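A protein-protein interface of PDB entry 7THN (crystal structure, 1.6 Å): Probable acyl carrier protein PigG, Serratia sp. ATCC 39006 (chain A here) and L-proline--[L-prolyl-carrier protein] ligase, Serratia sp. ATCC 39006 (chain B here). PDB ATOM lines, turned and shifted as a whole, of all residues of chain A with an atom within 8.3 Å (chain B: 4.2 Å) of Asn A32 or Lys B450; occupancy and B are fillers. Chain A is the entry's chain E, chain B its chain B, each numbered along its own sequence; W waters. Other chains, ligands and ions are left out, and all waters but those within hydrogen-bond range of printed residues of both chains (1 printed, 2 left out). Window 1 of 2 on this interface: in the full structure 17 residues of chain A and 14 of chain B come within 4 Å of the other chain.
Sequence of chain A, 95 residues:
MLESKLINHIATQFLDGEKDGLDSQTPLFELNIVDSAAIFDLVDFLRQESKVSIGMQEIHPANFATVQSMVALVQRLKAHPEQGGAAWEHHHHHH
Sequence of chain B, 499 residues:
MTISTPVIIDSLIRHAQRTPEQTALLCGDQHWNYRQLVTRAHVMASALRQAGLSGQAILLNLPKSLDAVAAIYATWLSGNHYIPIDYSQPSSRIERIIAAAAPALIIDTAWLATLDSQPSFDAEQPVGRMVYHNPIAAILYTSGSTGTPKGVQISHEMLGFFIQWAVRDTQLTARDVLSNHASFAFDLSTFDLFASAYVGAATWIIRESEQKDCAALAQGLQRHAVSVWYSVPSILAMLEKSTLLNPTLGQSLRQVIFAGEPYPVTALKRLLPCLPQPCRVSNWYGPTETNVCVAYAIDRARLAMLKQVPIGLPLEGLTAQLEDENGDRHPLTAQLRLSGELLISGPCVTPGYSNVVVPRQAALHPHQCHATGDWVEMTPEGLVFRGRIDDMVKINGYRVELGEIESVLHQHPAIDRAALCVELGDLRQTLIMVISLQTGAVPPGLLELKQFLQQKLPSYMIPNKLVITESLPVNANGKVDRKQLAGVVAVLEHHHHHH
The side-chain amino group of Lys B450 is in hydrogen-bond range of the backbone carbonyl oxygen of Leu A31, at 2.8 Å.
O of Asn A32 sits at hydrogen-bond distance from NZ of Lys B450, 3.2 Å away.
The side-chain amide nitrogen of Asn A32 lies within hydrogen-bond range of the backbone carbonyl oxygen of Ile B462 (2.8 Å).
ND2 of Asn B464 is in hydrogen-bond range of O of Phe A14, 3.0 Å away.
O of Asn A32 lies close to OD1 of Asn B464, at 3.2 Å.
O of Pro B463 is in hydrogen-bond range of NZ of Lys B450, at 2.9 Å.
NZ of Lys B450 sits at hydrogen-bond distance from OD1 of Asn B464 (2.8 Å).
O of Leu A28 lies within hydrogen-bond range of N of Ile A33 (2.9 Å).
CD2 of Leu B446 touches CD2 of Leu A15 (3.8 Å).
Leu A15 touches Asn B464 (CD2 to OD1, 3.9 Å).
O of Phe A29 touches CB of Ser B459, at 3.7 Å.
Gln B454 touches Glu A30 (NE2 to OE1, 3.7 Å).
O of Glu A30 touches CB of Ser B459, at 3.6 Å.
CD1 of Ile B462 touches O of Glu A30, 3.5 Å away.
CD2 of Leu A31 touches CB of Gln B454 (3.9 Å).
CG2 of Ile B462 touches O of Leu A31, 3.6 Å away.
O of Ser B459 touches CB of Asn A32, 3.2 Å away.
CA of Ile A33 touches OD1 of Asn B464, at 3.5 Å.
Lys B450 touches just these residues of chain A: Leu A31 (2.8 Å), Asn A32 (3.2 Å) and Ile A33 (3.9 Å).
Printed residues of chain B within 4 Å of Leu A15: Leu B446 and Asn B464.
Of the printed residues of chain B, Ile A33 touches Lys B450 (3.9 Å) and Asn B464 (3.5 Å).
Printed residues of chain A within 4 Å of Ser B459: Phe A29, Glu A30 and Asn A32.
Printed residues of chain B within 4 Å of Glu A30: Gln B454, Ser B459 and Ile B462.
Printed residues of chain A within 4 Å of Asn B464: Phe A14, Leu A15, Asn A32 and Ile A33.
Phe B452 touches none of the printed residues of chain A.
The nearest printed residue of chain B that does not touch Asn A32 is Pro B463 (5.0 Å).
The nearest residue of chain A that does not touch Lys B450 is Leu A15 (4.7 Å).
Printed residues of chain A that touch a printed residue of chain B: Phe A14, Leu A15, Phe A29, Glu A30, Leu A31, Asn A32 and Ile A33.
Hydrophobic or aromatic side chains of chain B within 4 Å of the printed part of chain A: Leu B446 and Ile B462.
Among the printed residues, 16 pairs touch across the chains.
Among the printed residues, no Asp or Glu carboxylate lies within 4 Å of a Lys or Arg side-chain nitrogen of the other chain.
Water W1 lies within hydrogen-bond range of the side-chain hydroxyl (OG1) of Thr A26 (3.1 Å) and the side-chain amide nitrogen (NE2) of Gln B451 (3.5 Å).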
ATOM      1  N   PHE A  14      -0.086  15.358  -2.553  1.00  0.00           N
ATOM      2  CA  PHE A  14       0.809  14.356  -3.203  1.00  0.00           C
ATOM      3  C   PHE A  14       2.278  14.767  -3.093  1.00  0.00           C
ATOM      4  O   PHE A  14       3.136  13.912  -3.263  1.00  0.00           O
ATOM      5  CB  PHE A  14       0.363  14.154  -4.655  1.00  0.00           C
ATOM      6  CG  PHE A  14      -1.009  13.562  -4.760  1.00  0.00           C
ATOM      7  CD1 PHE A  14      -1.236  12.240  -4.423  1.00  0.00           C
ATOM      8  CD2 PHE A  14      -2.085  14.339  -5.138  1.00  0.00           C
ATOM      9  CE1 PHE A  14      -2.507  11.700  -4.516  1.00  0.00           C
ATOM     10  CE2 PHE A  14      -3.359  13.806  -5.194  1.00  0.00           C
ATOM     11  CZ  PHE A  14      -3.563  12.483  -4.909  1.00  0.00           C
ATOM     12  N   LEU A  15       2.579  16.039  -2.890  1.00  0.00           N
ATOM     13  CA  LEU A  15       3.971  16.553  -2.954  1.00  0.00           C
ATOM     14  C   LEU A  15       4.347  17.291  -1.644  1.00  0.00           C
ATOM     15  O   LEU A  15       5.239  18.142  -1.699  1.00  0.00           O
ATOM     16  CB  LEU A  15       4.109  17.440  -4.193  1.00  0.00           C
ATOM     17  CG  LEU A  15       3.960  16.704  -5.541  1.00  0.00           C
ATOM     18  CD1 LEU A  15       3.939  17.687  -6.690  1.00  0.00           C
ATOM     19  CD2 LEU A  15       5.106  15.713  -5.727  1.00  0.00           C
ATOM     20  N   THR A  26       2.052  19.315 -16.118  1.00  0.00           N
ATOM     21  CA  THR A  26       2.801  18.217 -15.473  1.00  0.00           C
ATOM     22  C   THR A  26       2.008  16.916 -15.638  1.00  0.00           C
ATOM     23  O   THR A  26       0.876  16.854 -15.190  1.00  0.00           O
ATOM     24  CB  THR A  26       3.015  18.511 -13.989  1.00  0.00           C
ATOM     25  OG1 THR A  26       3.734  19.741 -13.858  1.00  0.00           O
ATOM     26  CG2 THR A  26       3.770  17.399 -13.296  1.00  0.00           C
ATOM     27  N   PRO A  27       2.587  15.862 -16.250  1.00  0.00           N
ATOM     28  CA  PRO A  27       1.917  14.560 -16.315  1.00  0.00           C
ATOM     29  C   PRO A  27       1.958  13.797 -14.980  1.00  0.00           C
ATOM     30  O   PRO A  27       2.945  13.203 -14.560  1.00  0.00           O
ATOM     31  CB  PRO A  27       2.629  13.887 -17.494  1.00  0.00           C
ATOM     32  CG  PRO A  27       3.995  14.482 -17.520  1.00  0.00           C
ATOM     33  CD  PRO A  27       3.866  15.883 -16.974  1.00  0.00           C
ATOM     34  N   LEU A  28       0.836  13.852 -14.301  1.00  0.00           N
ATOM     35  CA  LEU A  28       0.660  13.441 -12.893  1.00  0.00           C
ATOM     36  C   LEU A  28       0.917  11.943 -12.737  1.00  0.00           C
ATOM     37  O   LEU A  28       1.488  11.539 -11.704  1.00  0.00           O
ATOM     38  CB  LEU A  28      -0.735  13.829 -12.424  1.00  0.00           C
ATOM     39  CG  LEU A  28      -1.084  15.314 -12.470  1.00  0.00           C
ATOM     40  CD1 LEU A  28      -2.551  15.516 -12.182  1.00  0.00           C
ATOM     41  CD2 LEU A  28      -0.198  16.117 -11.513  1.00  0.00           C
ATOM     42  N   PHE A  29       0.430  11.122 -13.661  1.00  0.00           N
ATOM     43  CA  PHE A  29       0.575   9.648 -13.578  1.00  0.00           C
ATOM     44  C   PHE A  29       1.911   9.219 -14.187  1.00  0.00           C
ATOM     45  O   PHE A  29       2.593   8.364 -13.581  1.00  0.00           O
ATOM     46  CB  PHE A  29      -0.639   8.995 -14.236  1.00  0.00           C
ATOM     47  CG  PHE A  29      -1.915   9.257 -13.466  1.00  0.00           C
ATOM     48  CD1 PHE A  29      -2.243   8.487 -12.356  1.00  0.00           C
ATOM     49  CD2 PHE A  29      -2.691  10.368 -13.740  1.00  0.00           C
ATOM     50  CE1 PHE A  29      -3.406   8.743 -11.628  1.00  0.00           C
ATOM     51  CE2 PHE A  29      -3.826  10.649 -13.002  1.00  0.00           C
ATOM     52  CZ  PHE A  29      -4.191   9.827 -11.949  1.00  0.00           C
ATOM     53  N   GLU A  30       2.334   9.835 -15.291  1.00  0.00           N
ATOM     54  CA  GLU A  30       3.611   9.445 -15.942  1.00  0.00           C
ATOM     55  C   GLU A  30       4.791   9.682 -14.986  1.00  0.00           C
ATOM     56  O   GLU A  30       5.775   8.912 -15.043  1.00  0.00           O
ATOM     57  CB  GLU A  30       3.845  10.153 -17.272  1.00  0.00           C
ATOM     58  CG  GLU A  30       2.796   9.838 -18.320  1.00  0.00           C
ATOM     59  CD  GLU A  30       3.116  10.543 -19.633  1.00  0.00           C
ATOM     60  OE1 GLU A  30       4.317  10.511 -20.037  1.00  0.00           O
ATOM     61  OE2 GLU A  30       2.218  11.215 -20.189  1.00  0.00           O
ATOM     62  N   LEU A  31       4.717  10.727 -14.148  1.00  0.00           N
ATOM     63  CA  LEU A  31       5.810  11.042 -13.191  1.00  0.00           C
ATOM     64  C   LEU A  31       5.527  10.429 -11.810  1.00  0.00           C
ATOM     65  O   LEU A  31       6.352  10.649 -10.919  1.00  0.00           O
ATOM     66  CB  LEU A  31       6.027  12.552 -13.137  1.00  0.00           C
ATOM     67  CG  LEU A  31       6.485  13.198 -14.446  1.00  0.00           C
ATOM     68  CD1 LEU A  31       6.558  14.701 -14.313  1.00  0.00           C
ATOM     69  CD2 LEU A  31       7.798  12.644 -14.944  1.00  0.00           C
ATOM     70  N   ASN A  32       4.472   9.621 -11.669  1.00  0.00           N
ATOM     71  CA  ASN A  32       4.175   8.891 -10.413  1.00  0.00           C
ATOM     72  C   ASN A  32       3.999   9.899  -9.276  1.00  0.00           C
ATOM     73  O   ASN A  32       4.316   9.596  -8.095  1.00  0.00           O
ATOM     74  CB  ASN A  32       5.245   7.855 -10.076  1.00  0.00           C
ATOM     75  CG  ASN A  32       4.714   6.791  -9.141  1.00  0.00           C
ATOM     76  OD1 ASN A  32       3.511   6.503  -9.174  1.00  0.00           O
ATOM     77  ND2 ASN A  32       5.570   6.275  -8.260  1.00  0.00           N
ATOM     78  N   ILE A  33       3.434  11.060  -9.579  1.00  0.00           N
ATOM     79  CA  ILE A  33       2.995  12.025  -8.535  1.00  0.00           C
ATOM     80  C   ILE A  33       1.691  11.509  -7.932  1.00  0.00           C
ATOM     81  O   ILE A  33       1.539  11.503  -6.684  1.00  0.00           O
ATOM     82  CB  ILE A  33       2.854  13.427  -9.132  1.00  0.00           C
ATOM     83  CG1 ILE A  33       4.209  13.984  -9.561  1.00  0.00           C
ATOM     84  CG2 ILE A  33       2.172  14.369  -8.179  1.00  0.00           C
ATOM     85  CD1 ILE A  33       4.132  15.189 -10.461  1.00  0.00           C
ATOM     86  N   VAL A  34       0.810  11.038  -8.794  1.00  0.00           N
ATOM     87  CA  VAL A  34      -0.445  10.358  -8.370  1.00  0.00           C
ATOM     88  C   VAL A  34      -0.349   8.877  -8.775  1.00  0.00           C
ATOM     89  O   VAL A  34      -0.060   8.609  -9.930  1.00  0.00           O
ATOM     90  CB  VAL A  34      -1.666  11.026  -8.989  1.00  0.00           C
ATOM     91  CG1 VAL A  34      -2.914  10.351  -8.473  1.00  0.00           C
ATOM     92  CG2 VAL A  34      -1.717  12.519  -8.678  1.00  0.00           C
ATOM     93  N   ASP A  35      -0.505   7.981  -7.813  1.00  0.00           N
ATOM     94  CA  ASP A  35      -0.498   6.514  -8.062  1.00  0.00           C
ATOM     95  C   ASP A  35      -1.638   6.219  -9.026  1.00  0.00           C
ATOM     96  O   ASP A  35      -2.714   6.819  -8.889  1.00  0.00           O
ATOM     97  CB  ASP A  35      -0.621   5.757  -6.743  1.00  0.00           C
ATOM     98  CG  ASP A  35      -0.434   4.246  -6.841  1.00  0.00           C
ATOM     99  OD1 ASP A  35      -1.139   3.596  -7.604  1.00  0.00           O
ATOM    100  OD2 ASP A  35       0.394   3.743  -6.112  1.00  0.00           O
ATOM    101  N   SER A  36      -1.409   5.364 -10.018  1.00  0.00           N
ATOM    102  CA  SER A  36      -2.468   4.937 -10.960  1.00  0.00           C
ATOM    103  C   SER A  36      -3.691   4.478 -10.176  1.00  0.00           C
ATOM    104  O   SER A  36      -4.849   4.742 -10.600  1.00  0.00           O
ATOM    105  CB  SER A  36      -1.991   3.883 -11.924  1.00  0.00           C
ATOM    106  OG  SER A  36      -1.349   2.825 -11.268  1.00  0.00           O
ATOM    107  N   ALA A  37      -3.471   3.867  -9.021  1.00  0.00           N
ATOM    108  CA  ALA A  37      -4.548   3.287  -8.222  1.00  0.00           C
ATOM    109  C   ALA A  37      -5.323   4.354  -7.468  1.00  0.00           C
ATOM    110  O   ALA A  37      -6.390   3.987  -6.998  1.00  0.00           O
ATOM    111  CB  ALA A  37      -4.001   2.233  -7.285  1.00  0.00           C
ATOM    112  N   LEU B 446      12.750  17.303  -6.809  1.00  0.00           N
ATOM    113  CA  LEU B 446      11.971  16.048  -6.962  1.00  0.00           C
ATOM    114  C   LEU B 446      11.454  15.910  -8.396  1.00  0.00           C
ATOM    115  O   LEU B 446      11.675  14.819  -9.012  1.00  0.00           O
ATOM    116  CB  LEU B 446      10.825  16.031  -5.965  1.00  0.00           C
ATOM    117  CG  LEU B 446       9.927  14.803  -6.039  1.00  0.00           C
ATOM    118  CD1 LEU B 446      10.721  13.518  -5.833  1.00  0.00           C
ATOM    119  CD2 LEU B 446       8.782  14.918  -5.025  1.00  0.00           C
ATOM    120  N   LEU B 447      10.766  16.910  -8.944  1.00  0.00           N
ATOM    121  CA  LEU B 447      10.182  16.761 -10.312  1.00  0.00           C
ATOM    122  C   LEU B 447      11.307  16.600 -11.349  1.00  0.00           C
ATOM    123  O   LEU B 447      11.110  15.840 -12.322  1.00  0.00           O
ATOM    124  CB  LEU B 447       9.172  17.879 -10.609  1.00  0.00           C
ATOM    125  CG  LEU B 447       7.712  17.480 -10.350  1.00  0.00           C
ATOM    126  CD1 LEU B 447       7.460  17.043  -8.913  1.00  0.00           C
ATOM    127  CD2 LEU B 447       6.740  18.594 -10.746  1.00  0.00           C
ATOM    128  N   GLU B 448      12.459  17.273 -11.173  1.00  0.00           N
ATOM    129  CA  GLU B 448      13.600  17.112 -12.100  1.00  0.00           C
ATOM    130  C   GLU B 448      14.062  15.648 -12.078  1.00  0.00           C
ATOM    131  O   GLU B 448      14.346  15.085 -13.150  1.00  0.00           O
ATOM    132  CB  GLU B 448      14.730  18.073 -11.738  1.00  0.00           C
ATOM    133  CG  GLU B 448      14.362  19.496 -12.067  1.00  0.00           C
ATOM    134  CD  GLU B 448      15.335  20.538 -11.547  1.00  0.00           C
ATOM    135  OE1 GLU B 448      16.118  20.194 -10.637  1.00  0.00           O
ATOM    136  OE2 GLU B 448      15.318  21.685 -12.094  1.00  0.00           O
ATOM    137  N   LEU B 449      14.160  15.028 -10.909  1.00  0.00           N
ATOM    138  CA  LEU B 449      14.622  13.628 -10.862  1.00  0.00           C
ATOM    139  C   LEU B 449      13.545  12.725 -11.436  1.00  0.00           C
ATOM    140  O   LEU B 449      13.902  11.726 -12.092  1.00  0.00           O
ATOM    141  CB  LEU B 449      14.961  13.225  -9.439  1.00  0.00           C
ATOM    142  CG  LEU B 449      16.248  13.814  -8.889  1.00  0.00           C
ATOM    143  CD1 LEU B 449      16.472  13.257  -7.514  1.00  0.00           C
ATOM    144  CD2 LEU B 449      17.436  13.523  -9.797  1.00  0.00           C
ATOM    145  N   LYS B 450      12.273  13.017 -11.172  1.00  0.00           N
ATOM    146  CA  LYS B 450      11.207  12.180 -11.792  1.00  0.00           C
ATOM    147  C   LYS B 450      11.318  12.256 -13.311  1.00  0.00           C
ATOM    148  O   LYS B 450      11.134  11.228 -13.957  1.00  0.00           O
ATOM    149  CB  LYS B 450       9.841  12.671 -11.356  1.00  0.00           C
ATOM    150  CG  LYS B 450       9.488  12.415  -9.893  1.00  0.00           C
ATOM    151  CD  LYS B 450       8.172  13.087  -9.539  1.00  0.00           C
ATOM    152  CE  LYS B 450       7.580  12.637  -8.216  1.00  0.00           C
ATOM    153  NZ  LYS B 450       7.096  11.229  -8.273  1.00  0.00           N
ATOM    154  N   GLN B 451      11.578  13.437 -13.865  1.00  0.00           N
ATOM    155  CA  GLN B 451      11.709  13.620 -15.339  1.00  0.00           C
ATOM    156  C   GLN B 451      12.942  12.873 -15.852  1.00  0.00           C
ATOM    157  O   GLN B 451      12.882  12.292 -16.984  1.00  0.00           O
ATOM    158  CB  GLN B 451      11.825  15.113 -15.680  1.00  0.00           C
ATOM    159  CG  GLN B 451      10.513  15.858 -15.453  1.00  0.00           C
ATOM    160  CD  GLN B 451      10.647  17.359 -15.564  1.00  0.00           C
ATOM    161  OE1 GLN B 451      11.690  17.937 -15.220  1.00  0.00           O
ATOM    162  NE2 GLN B 451       9.589  17.991 -16.052  1.00  0.00           N
ATOM    163  N   PHE B 452      14.011  12.829 -15.057  1.00  0.00           N
ATOM    164  CA  PHE B 452      15.243  12.082 -15.398  1.00  0.00           C
ATOM    165  C   PHE B 452      14.932  10.585 -15.519  1.00  0.00           C
ATOM    166  O   PHE B 452      15.393   9.923 -16.486  1.00  0.00           O
ATOM    167  CB  PHE B 452      16.328  12.347 -14.353  1.00  0.00           C
ATOM    168  CG  PHE B 452      17.577  11.523 -14.492  1.00  0.00           C
ATOM    169  CD1 PHE B 452      18.572  11.863 -15.398  1.00  0.00           C
ATOM    170  CD2 PHE B 452      17.799  10.442 -13.666  1.00  0.00           C
ATOM    171  CE1 PHE B 452      19.736  11.097 -15.484  1.00  0.00           C
ATOM    172  CE2 PHE B 452      18.958   9.692 -13.747  1.00  0.00           C
ATOM    173  CZ  PHE B 452      19.935  10.026 -14.647  1.00  0.00           C
ATOM    174  N   LEU B 453      14.140  10.067 -14.585  1.00  0.00           N
ATOM    175  CA  LEU B 453      13.819   8.624 -14.531  1.00  0.00           C
ATOM    176  C   LEU B 453      12.753   8.260 -15.543  1.00  0.00           C
ATOM    177  O   LEU B 453      12.729   7.109 -15.948  1.00  0.00           O
ATOM    178  CB  LEU B 453      13.349   8.249 -13.135  1.00  0.00           C
ATOM    179  CG  LEU B 453      14.426   8.347 -12.073  1.00  0.00           C
ATOM    180  CD1 LEU B 453      13.857   7.984 -10.706  1.00  0.00           C
ATOM    181  CD2 LEU B 453      15.642   7.486 -12.422  1.00  0.00           C
ATOM    182  N   GLN B 454      11.916   9.199 -15.940  1.00  0.00           N
ATOM    183  CA  GLN B 454      10.775   8.914 -16.844  1.00  0.00           C
ATOM    184  C   GLN B 454      11.226   8.301 -18.180  1.00  0.00           C
ATOM    185  O   GLN B 454      10.458   7.508 -18.743  1.00  0.00           O
ATOM    186  CB  GLN B 454       9.982  10.201 -17.034  1.00  0.00           C
ATOM    187  CG  GLN B 454       8.678   9.977 -17.773  1.00  0.00           C
ATOM    188  CD  GLN B 454       8.864  10.066 -19.261  1.00  0.00           C
ATOM    189  OE1 GLN B 454       9.824  10.659 -19.735  1.00  0.00           O
ATOM    190  NE2 GLN B 454       7.923   9.507 -19.994  1.00  0.00           N
ATOM    191  N   SER B 459       6.783   3.980 -14.771  1.00  0.00           N
ATOM    192  CA  SER B 459       6.276   4.997 -13.831  1.00  0.00           C
ATOM    193  C   SER B 459       6.273   4.482 -12.399  1.00  0.00           C
ATOM    194  O   SER B 459       6.561   5.274 -11.499  1.00  0.00           O
ATOM    195  CB  SER B 459       4.929   5.501 -14.211  1.00  0.00           C
ATOM    196  OG  SER B 459       3.978   4.442 -14.199  1.00  0.00           O
ATOM    197  N   ILE B 462       9.362   5.203 -10.301  1.00  0.00           N
ATOM    198  CA  ILE B 462       9.774   6.619 -10.134  1.00  0.00           C
ATOM    199  C   ILE B 462       9.414   7.066  -8.722  1.00  0.00           C
ATOM    200  O   ILE B 462       8.243   7.215  -8.381  1.00  0.00           O
ATOM    201  CB  ILE B 462       9.158   7.518 -11.214  1.00  0.00           C
ATOM    202  CG1 ILE B 462       9.510   7.041 -12.617  1.00  0.00           C
ATOM    203  CG2 ILE B 462       9.575   8.962 -10.959  1.00  0.00           C
ATOM    204  CD1 ILE B 462       8.851   7.831 -13.727  1.00  0.00           C
ATOM    205  N   PRO B 463      10.400   7.316  -7.835  1.00  0.00           N
ATOM    206  CA  PRO B 463      10.067   7.627  -6.452  1.00  0.00           C
ATOM    207  C   PRO B 463       9.286   8.913  -6.270  1.00  0.00           C
ATOM    208  O   PRO B 463       9.323   9.784  -7.147  1.00  0.00           O
ATOM    209  CB  PRO B 463      11.434   7.686  -5.746  1.00  0.00           C
ATOM    210  CG  PRO B 463      12.291   6.800  -6.606  1.00  0.00           C
ATOM    211  CD  PRO B 463      11.845   7.135  -8.032  1.00  0.00           C
ATOM    212  N   ASN B 464       8.563   9.028  -5.152  1.00  0.00           N
ATOM    213  CA  ASN B 464       7.726  10.222  -4.944  1.00  0.00           C
ATOM    214  C   ASN B 464       8.207  11.070  -3.766  1.00  0.00           C
ATOM    215  O   ASN B 464       7.523  12.022  -3.455  1.00  0.00           O
ATOM    216  CB  ASN B 464       6.226   9.923  -4.796  1.00  0.00           C
ATOM    217  CG  ASN B 464       5.350  11.130  -5.093  1.00  0.00           C
ATOM    218  OD1 ASN B 464       5.518  11.826  -6.080  1.00  0.00           O
ATOM    219  ND2 ASN B 464       4.341  11.389  -4.253  1.00  0.00           N
HETATM  220  O   HOH W   1       6.276  18.778 -15.285  1.00  0.00           O
